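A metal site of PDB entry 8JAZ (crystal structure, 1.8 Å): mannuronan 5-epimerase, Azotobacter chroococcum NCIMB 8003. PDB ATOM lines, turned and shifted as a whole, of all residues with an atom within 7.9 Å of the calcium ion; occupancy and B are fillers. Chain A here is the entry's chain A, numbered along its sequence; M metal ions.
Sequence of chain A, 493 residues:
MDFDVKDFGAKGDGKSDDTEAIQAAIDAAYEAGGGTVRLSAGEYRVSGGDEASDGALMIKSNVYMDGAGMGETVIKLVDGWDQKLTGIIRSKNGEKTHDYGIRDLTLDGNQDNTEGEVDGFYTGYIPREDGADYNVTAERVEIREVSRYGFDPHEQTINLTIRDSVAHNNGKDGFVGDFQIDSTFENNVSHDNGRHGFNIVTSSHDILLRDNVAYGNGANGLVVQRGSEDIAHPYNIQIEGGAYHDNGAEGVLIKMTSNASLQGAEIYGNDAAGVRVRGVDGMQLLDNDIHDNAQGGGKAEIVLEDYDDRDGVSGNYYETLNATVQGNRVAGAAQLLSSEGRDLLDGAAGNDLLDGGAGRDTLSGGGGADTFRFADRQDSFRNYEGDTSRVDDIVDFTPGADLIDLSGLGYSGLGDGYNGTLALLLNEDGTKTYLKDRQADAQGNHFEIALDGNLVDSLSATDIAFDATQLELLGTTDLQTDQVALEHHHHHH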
ATOM      1  N   MET A  58      -1.739  -1.459   6.243  1.00  0.00           N
ATOM      2  CA  MET A  58      -2.619  -2.274   5.404  1.00  0.00           C
ATOM      3  C   MET A  58      -2.216  -3.729   5.606  1.00  0.00           C
ATOM      4  O   MET A  58      -1.268  -4.215   4.985  1.00  0.00           O
ATOM      5  CB  MET A  58      -2.508  -1.853   3.948  1.00  0.00           C
ATOM      6  CG  MET A  58      -3.568  -2.440   3.028  1.00  0.00           C
ATOM      7  SD  MET A  58      -5.238  -1.959   3.511  1.00  0.00           S
ATOM      8  CE  MET A  58      -5.307  -0.278   2.881  1.00  0.00           C
ATOM      9  N   ILE A  59      -2.935  -4.425   6.486  1.00  0.00           N
ATOM     10  CA  ILE A  59      -2.680  -5.845   6.714  1.00  0.00           C
ATOM     11  C   ILE A  59      -3.246  -6.652   5.551  1.00  0.00           C
ATOM     12  O   ILE A  59      -4.211  -6.234   4.908  1.00  0.00           O
ATOM     13  CB  ILE A  59      -3.252  -6.320   8.065  1.00  0.00           C
ATOM     14  CG1 ILE A  59      -2.585  -7.636   8.485  1.00  0.00           C
ATOM     15  CG2 ILE A  59      -4.765  -6.461   7.996  1.00  0.00           C
ATOM     16  CD1 ILE A  59      -2.862  -8.035   9.919  1.00  0.00           C
ATOM     17  N   SER A  61      -3.722 -10.760   3.402  1.00  0.00           N
ATOM     18  CA  SER A  61      -4.068 -12.168   3.553  1.00  0.00           C
ATOM     19  C   SER A  61      -2.879 -13.019   3.991  1.00  0.00           C
ATOM     20  O   SER A  61      -1.774 -12.868   3.467  1.00  0.00           O
ATOM     21  CB  SER A  61      -4.654 -12.723   2.255  1.00  0.00           C
ATOM     22  OG  SER A  61      -5.763 -11.950   1.824  1.00  0.00           O
ATOM     23  N   ARG A  90      -5.906  -2.134   9.034  1.00  0.00           N
ATOM     24  CA  ARG A  90      -7.101  -2.435   8.267  1.00  0.00           C
ATOM     25  C   ARG A  90      -6.732  -3.297   7.072  1.00  0.00           C
ATOM     26  O   ARG A  90      -5.563  -3.396   6.687  1.00  0.00           O
ATOM     27  CB  ARG A  90      -7.825  -1.164   7.798  1.00  0.00           C
ATOM     28  CG  ARG A  90      -7.082  -0.402   6.709  1.00  0.00           C
ATOM     29  CD  ARG A  90      -7.973   0.656   6.067  1.00  0.00           C
ATOM     30  NE  ARG A  90      -9.026   0.070   5.244  1.00  0.00           N
ATOM     31  CZ  ARG A  90     -10.199   0.645   5.006  1.00  0.00           C
ATOM     32  NH1 ARG A  90     -10.518   1.812   5.535  1.00  0.00           N
ATOM     33  NH2 ARG A  90     -11.077   0.024   4.221  1.00  0.00           N
ATOM     34  N   SER A  91      -7.750  -3.932   6.502  1.00  0.00           N
ATOM     35  CA  SER A  91      -7.605  -4.644   5.243  1.00  0.00           C
ATOM     36  C   SER A  91      -8.024  -3.715   4.106  1.00  0.00           C
ATOM     37  O   SER A  91      -8.556  -2.638   4.348  1.00  0.00           O
ATOM     38  CB  SER A  91      -8.438  -5.935   5.240  1.00  0.00           C
ATOM     39  OG  SER A  91      -9.798  -5.658   4.989  1.00  0.00           O
ATOM     40  N   MLY A  92      -7.786  -4.138   2.868  1.00  0.00           N
ATOM     41  CA  MLY A  92      -8.056  -3.277   1.720  1.00  0.00           C
ATOM     42  CB  MLY A  92      -7.227  -3.712   0.508  1.00  0.00           C
ATOM     43  CG  MLY A  92      -7.353  -2.788  -0.691  1.00  0.00           C
ATOM     44  CD  MLY A  92      -6.710  -3.384  -1.938  1.00  0.00           C
ATOM     45  CE  MLY A  92      -6.547  -2.329  -3.021  1.00  0.00           C
ATOM     46  NZ  MLY A  92      -6.072  -2.871  -4.339  1.00  0.00           N
ATOM     47  CH1 MLY A  92      -7.190  -3.603  -4.927  1.00  0.00           C
ATOM     48  CH2 MLY A  92      -5.002  -3.847  -4.082  1.00  0.00           C
ATOM     49  C   MLY A  92      -9.540  -3.248   1.336  1.00  0.00           C
ATOM     50  O   MLY A  92     -10.235  -4.262   1.431  1.00  0.00           O
ATOM     51  N   ASN A  93     -10.060  -2.050   1.096  1.00  0.00           N
ATOM     52  CA  ASN A  93     -11.412  -1.902   0.575  1.00  0.00           C
ATOM     53  C   ASN A  93     -11.444  -2.495  -0.828  1.00  0.00           C
ATOM     54  O   ASN A  93     -10.545  -2.261  -1.635  1.00  0.00           O
ATOM     55  CB  ASN A  93     -11.829  -0.425   0.560  1.00  0.00           C
ATOM     56  CG  ASN A  93     -13.229  -0.206   0.029  1.00  0.00           C
ATOM     57  OD1 ASN A  93     -13.487  -0.358  -1.167  1.00  0.00           O
ATOM     58  ND2 ASN A  93     -14.148   0.156   0.914  1.00  0.00           N
ATOM     59  N   GLY A  94     -12.480  -3.279  -1.129  1.00  0.00           N
ATOM     60  CA  GLY A  94     -12.600  -3.915  -2.414  1.00  0.00           C
ATOM     61  C   GLY A  94     -11.823  -5.206  -2.568  1.00  0.00           C
ATOM     62  O   GLY A  94     -11.696  -5.714  -3.684  1.00  0.00           O
ATOM     63  N   GLU A  95     -11.286  -5.750  -1.472  1.00  0.00           N
ATOM     64  CA  GLU A  95     -10.559  -7.006  -1.521  1.00  0.00           C
ATOM     65  C   GLU A  95     -11.086  -7.927  -0.422  1.00  0.00           C
ATOM     66  O   GLU A  95     -11.320  -7.489   0.696  1.00  0.00           O
ATOM     67  CB  GLU A  95      -9.056  -6.781  -1.366  1.00  0.00           C
ATOM     68  CG  GLU A  95      -8.253  -8.058  -1.132  1.00  0.00           C
ATOM     69  CD  GLU A  95      -6.822  -7.782  -0.705  1.00  0.00           C
ATOM     70  OE1 GLU A  95      -6.018  -7.342  -1.556  1.00  0.00           O
ATOM     71  OE2 GLU A  95      -6.496  -8.003   0.485  1.00  0.00           O
ATOM     72  N   MLY A  96     -11.273  -9.193  -0.758  1.00  0.00           N
ATOM     73  CA  MLY A  96     -11.783 -10.166   0.203  1.00  0.00           C
ATOM     74  CB  MLY A  96     -12.593 -11.237  -0.512  1.00  0.00           C
ATOM     75  CG  MLY A  96     -13.853 -10.687  -1.158  1.00  0.00           C
ATOM     76  CD  MLY A  96     -14.359 -11.559  -2.281  1.00  0.00           C
ATOM     77  CE  MLY A  96     -15.548 -10.929  -2.989  1.00  0.00           C
ATOM     78  NZ  MLY A  96     -16.150 -11.829  -4.008  1.00  0.00           N
ATOM     79  CH1 MLY A  96     -17.088 -12.710  -3.308  1.00  0.00           C
ATOM     80  CH2 MLY A  96     -16.951 -10.963  -4.878  1.00  0.00           C
ATOM     81  C   MLY A  96     -10.642 -10.789   1.011  1.00  0.00           C
ATOM     82  O   MLY A  96     -10.026 -11.756   0.563  1.00  0.00           O
ATOM     83  N   THR A  97      -9.942  -9.926   1.749  1.00  0.00           N
ATOM     84  CA  THR A  97      -8.816 -10.320   2.581  1.00  0.00           C
ATOM     85  C   THR A  97      -9.215 -11.429   3.547  1.00  0.00           C
ATOM     86  O   THR A  97     -10.327 -11.444   4.053  1.00  0.00           O
ATOM     87  CB  THR A  97      -8.276  -9.123   3.380  1.00  0.00           C
ATOM     88  OG1 THR A  97      -8.356  -7.940   2.581  1.00  0.00           O
ATOM     89  CG2 THR A  97      -6.830  -9.352   3.779  1.00  0.00           C
ATOM     90  N   HIS A  98      -8.303 -12.376   3.802  1.00  0.00           N
ATOM     91  CA  HIS A  98      -8.672 -13.546   4.579  1.00  0.00           C
ATOM     92  C   HIS A  98      -7.478 -14.060   5.371  1.00  0.00           C
ATOM     93  O   HIS A  98      -6.314 -13.828   5.023  1.00  0.00           O
ATOM     94  CB  HIS A  98      -9.207 -14.663   3.691  1.00  0.00           C
ATOM     95  CG  HIS A  98      -8.199 -15.205   2.714  1.00  0.00           C
ATOM     96  ND1 HIS A  98      -7.419 -16.298   2.990  1.00  0.00           N
ATOM     97  CD2 HIS A  98      -7.834 -14.779   1.478  1.00  0.00           C
ATOM     98  CE1 HIS A  98      -6.619 -16.539   1.968  1.00  0.00           C
ATOM     99  NE2 HIS A  98      -6.852 -15.637   1.033  1.00  0.00           N
ATOM    100  N   TYR A 100      -6.162 -13.438   8.450  1.00  0.00           N
ATOM    101  CA  TYR A 100      -5.242 -12.477   9.043  1.00  0.00           C
ATOM    102  C   TYR A 100      -5.720 -12.116  10.442  1.00  0.00           C
ATOM    103  O   TYR A 100      -6.847 -12.437  10.846  1.00  0.00           O
ATOM    104  CB  TYR A 100      -5.111 -11.214   8.176  1.00  0.00           C
ATOM    105  CG  TYR A 100      -6.375 -10.393   8.053  1.00  0.00           C
ATOM    106  CD1 TYR A 100      -7.318 -10.683   7.079  1.00  0.00           C
ATOM    107  CD2 TYR A 100      -6.597  -9.313   8.890  1.00  0.00           C
ATOM    108  CE1 TYR A 100      -8.465  -9.924   6.949  1.00  0.00           C
ATOM    109  CE2 TYR A 100      -7.741  -8.545   8.772  1.00  0.00           C
ATOM    110  CZ  TYR A 100      -8.670  -8.855   7.799  1.00  0.00           C
ATOM    111  OH  TYR A 100      -9.813  -8.098   7.679  1.00  0.00           O
ATOM    112  N   TYR A 122     -10.058  -2.090  11.423  1.00  0.00           N
ATOM    113  CA  TYR A 122     -11.147  -2.055  10.458  1.00  0.00           C
ATOM    114  C   TYR A 122     -11.013  -3.215   9.480  1.00  0.00           C
ATOM    115  O   TYR A 122      -9.915  -3.477   8.965  1.00  0.00           O
ATOM    116  CB  TYR A 122     -11.158  -0.722   9.699  1.00  0.00           C
ATOM    117  CG  TYR A 122     -12.405  -0.470   8.862  1.00  0.00           C
ATOM    118  CD1 TYR A 122     -12.517  -1.003   7.581  1.00  0.00           C
ATOM    119  CD2 TYR A 122     -13.443   0.303   9.351  1.00  0.00           C
ATOM    120  CE1 TYR A 122     -13.651  -0.769   6.825  1.00  0.00           C
ATOM    121  CE2 TYR A 122     -14.577   0.537   8.595  1.00  0.00           C
ATOM    122  CZ  TYR A 122     -14.672   0.003   7.328  1.00  0.00           C
ATOM    123  OH  TYR A 122     -15.793   0.227   6.575  1.00  0.00           O
ATOM    124  N   THR A 123     -12.117  -3.913   9.234  1.00  0.00           N
ATOM    125  CA  THR A 123     -12.171  -5.034   8.291  1.00  0.00           C
ATOM    126  C   THR A 123     -13.387  -4.859   7.394  1.00  0.00           C
ATOM    127  O   THR A 123     -14.228  -3.987   7.626  1.00  0.00           O
ATOM    128  CB  THR A 123     -12.238  -6.385   9.014  1.00  0.00           C
ATOM    129  OG1 THR A 123     -13.578  -6.630   9.460  1.00  0.00           O
ATOM    130  CG2 THR A 123     -11.299  -6.430  10.220  1.00  0.00           C
ATOM    131  N   GLY A 124     -13.476  -5.674   6.353  1.00  0.00           N
ATOM    132  CA  GLY A 124     -14.612  -5.700   5.464  1.00  0.00           C
ATOM    133  C   GLY A 124     -14.208  -5.595   4.012  1.00  0.00           C
ATOM    134  O   GLY A 124     -13.040  -5.427   3.674  1.00  0.00           O
ATOM    135  N   TYR A 125     -15.204  -5.715   3.134  1.00  0.00           N
ATOM    136  CA  TYR A 125     -14.941  -5.688   1.709  1.00  0.00           C
ATOM    137  C   TYR A 125     -15.323  -4.364   1.055  1.00  0.00           C
ATOM    138  O   TYR A 125     -14.443  -3.599   0.647  1.00  0.00           O
ATOM    139  CB  TYR A 125     -15.695  -6.847   1.043  1.00  0.00           C
ATOM    140  CG  TYR A 125     -15.643  -6.880  -0.467  1.00  0.00           C
ATOM    141  CD1 TYR A 125     -16.768  -6.563  -1.224  1.00  0.00           C
ATOM    142  CD2 TYR A 125     -14.486  -7.246  -1.147  1.00  0.00           C
ATOM    143  CE1 TYR A 125     -16.739  -6.594  -2.602  1.00  0.00           C
ATOM    144  CE2 TYR A 125     -14.447  -7.285  -2.531  1.00  0.00           C
ATOM    145  CZ  TYR A 125     -15.580  -6.957  -3.249  1.00  0.00           C
ATOM    146  OH  TYR A 125     -15.550  -6.998  -4.629  1.00  0.00           O
ATOM    147  N   ILE A 126     -16.619  -4.066   1.022  1.00  0.00           N
ATOM    148  CA  ILE A 126     -17.183  -2.819   0.479  1.00  0.00           C
ATOM    149  C   ILE A 126     -18.549  -2.585   1.128  1.00  0.00           C
ATOM    150  O   ILE A 126     -19.371  -3.518   1.183  1.00  0.00           O
ATOM    151  CB  ILE A 126     -17.340  -2.842  -1.059  1.00  0.00           C
ATOM    152  CG1 ILE A 126     -16.029  -3.092  -1.798  1.00  0.00           C
ATOM    153  CG2 ILE A 126     -17.944  -1.529  -1.540  1.00  0.00           C
ATOM    154  CD1 ILE A 126     -16.188  -3.277  -3.296  1.00  0.00           C
ATOM    155  N   ALA A 132     -16.865 -10.474   1.225  1.00  0.00           N
ATOM    156  CA  ALA A 132     -16.573 -10.385   2.638  1.00  0.00           C
ATOM    157  C   ALA A 132     -15.133 -10.791   2.899  1.00  0.00           C
ATOM    158  O   ALA A 132     -14.575 -11.662   2.217  1.00  0.00           O
ATOM    159  CB  ALA A 132     -17.515 -11.260   3.463  1.00  0.00           C
ATOM    160  N   ASP A 133     -14.532 -10.152   3.896  1.00  0.00           N
ATOM    161  CA  ASP A 133     -13.376 -10.726   4.573  1.00  0.00           C
ATOM    162  C   ASP A 133     -13.809 -11.978   5.319  1.00  0.00           C
ATOM    163  O   ASP A 133     -14.964 -12.117   5.724  1.00  0.00           O
ATOM    164  CB  ASP A 133     -12.777  -9.715   5.547  1.00  0.00           C
ATOM    165  CG  ASP A 133     -11.928  -8.659   4.860  1.00  0.00           C
ATOM    166  OD1 ASP A 133     -11.872  -8.663   3.608  1.00  0.00           O
ATOM    167  OD2 ASP A 133     -11.336  -7.818   5.565  1.00  0.00           O
ATOM    168  N   TYR A 134     -12.872 -12.899   5.513  1.00  0.00           N
ATOM    169  CA  TYR A 134     -13.195 -14.109   6.251  1.00  0.00           C
ATOM    170  C   TYR A 134     -11.974 -14.594   7.014  1.00  0.00           C
ATOM    171  O   TYR A 134     -10.833 -14.363   6.610  1.00  0.00           O
ATOM    172  CB  TYR A 134     -13.761 -15.215   5.346  1.00  0.00           C
ATOM    173  CG  TYR A 134     -12.981 -15.521   4.090  1.00  0.00           C
ATOM    174  CD1 TYR A 134     -13.008 -14.664   3.001  1.00  0.00           C
ATOM    175  CD2 TYR A 134     -12.237 -16.702   3.980  1.00  0.00           C
ATOM    176  CE1 TYR A 134     -12.303 -14.954   1.835  1.00  0.00           C
ATOM    177  CE2 TYR A 134     -11.537 -16.995   2.827  1.00  0.00           C
ATOM    178  CZ  TYR A 134     -11.570 -16.121   1.755  1.00  0.00           C
ATOM    179  OH  TYR A 134     -10.871 -16.415   0.602  1.00  0.00           O
ATOM    180  N   GLU A 155     -18.547  -4.291   7.022  1.00  0.00           N
ATOM    181  CA  GLU A 155     -19.327  -5.074   6.067  1.00  0.00           C
ATOM    182  C   GLU A 155     -18.460  -5.490   4.875  1.00  0.00           C
ATOM    183  O   GLU A 155     -17.864  -4.642   4.208  1.00  0.00           O
ATOM    184  CB  GLU A 155     -20.517  -4.238   5.595  1.00  0.00           C
ATOM    185  CG  GLU A 155     -21.313  -4.865   4.475  1.00  0.00           C
ATOM    186  CD  GLU A 155     -22.417  -3.955   3.977  1.00  0.00           C
ATOM    187  OE1 GLU A 155     -23.039  -4.291   2.942  1.00  0.00           O
ATOM    188  OE2 GLU A 155     -22.646  -2.904   4.602  1.00  0.00           O
ATOM    189  N   GLN A 156     -18.389  -6.794   4.618  1.00  0.00           N
ATOM    190  CA  GLN A 156     -18.861  -7.894   5.464  1.00  0.00           C
ATOM    191  C   GLN A 156     -17.651  -8.625   6.023  1.00  0.00           C
ATOM    192  O   GLN A 156     -16.579  -8.585   5.428  1.00  0.00           O
ATOM    193  CB  GLN A 156     -19.735  -8.874   4.682  1.00  0.00           C
ATOM    194  CG  GLN A 156     -21.057  -8.346   4.169  1.00  0.00           C
ATOM    195  CD  GLN A 156     -21.794  -9.390   3.350  1.00  0.00           C
ATOM    196  OE1 GLN A 156     -21.592 -10.594   3.506  1.00  0.00           O
ATOM    197  NE2 GLN A 156     -22.663  -8.922   2.452  1.00  0.00           N
ATOM    198  N   THR A 157     -17.819  -9.292   7.164  1.00  0.00           N
ATOM    199  CA  THR A 157     -16.760 -10.125   7.717  1.00  0.00           C
ATOM    200  C   THR A 157     -17.361 -11.440   8.217  1.00  0.00           C
ATOM    201  O   THR A 157     -18.347 -11.432   8.959  1.00  0.00           O
ATOM    202  CB  THR A 157     -16.025  -9.413   8.855  1.00  0.00           C
ATOM    203  OG1 THR A 157     -15.601  -8.119   8.396  1.00  0.00           O
ATOM    204  CG2 THR A 157     -14.816 -10.208   9.283  1.00  0.00           C
HETATM  205 CA    CA M   1     -10.760  -6.418   2.559  1.00  0.00          CA
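The side-chain carboxylate of Asp 133 is in hydrogen-bond range of the side-chain hydroxyl of Tyr 100 (2.6 Å). O of Gln 156 lies within hydrogen-bond range of N of Asp 133. The backbone NH (N) of Tyr 134 lies within hydrogen-bond range of the backbone carbonyl oxygen (O) of Thr 97. N of Ser 91 sits at hydrogen-bond distance from O of Tyr 122, 3.3 Å away. N of MLY 92 lies within hydrogen-bond range of the side-chain sulfur of Met 58, at 3.4 Å.
Within 4 Å of the calcium ion: Ser 91, MLY 92, Glu 95, Thr 97, Gly 124 and Asp 133. Along chain A the residues within 4 Å of the calcium ion span positions 91 to 133. The nearest printed residue that does not touch the calcium ion is Tyr 125 (4.3 Å).
The calcium ion is bound by the backbone carbonyl oxygen (O) of Glu 95, O of MLY 92, the side-chain carboxylate (OD1) of Asp 133, the side-chain hydroxyl (OG) of Ser 91, the backbone carbonyl oxygen (O) of Gly 124 and the side-chain hydroxyl (OG1) of Thr 97.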
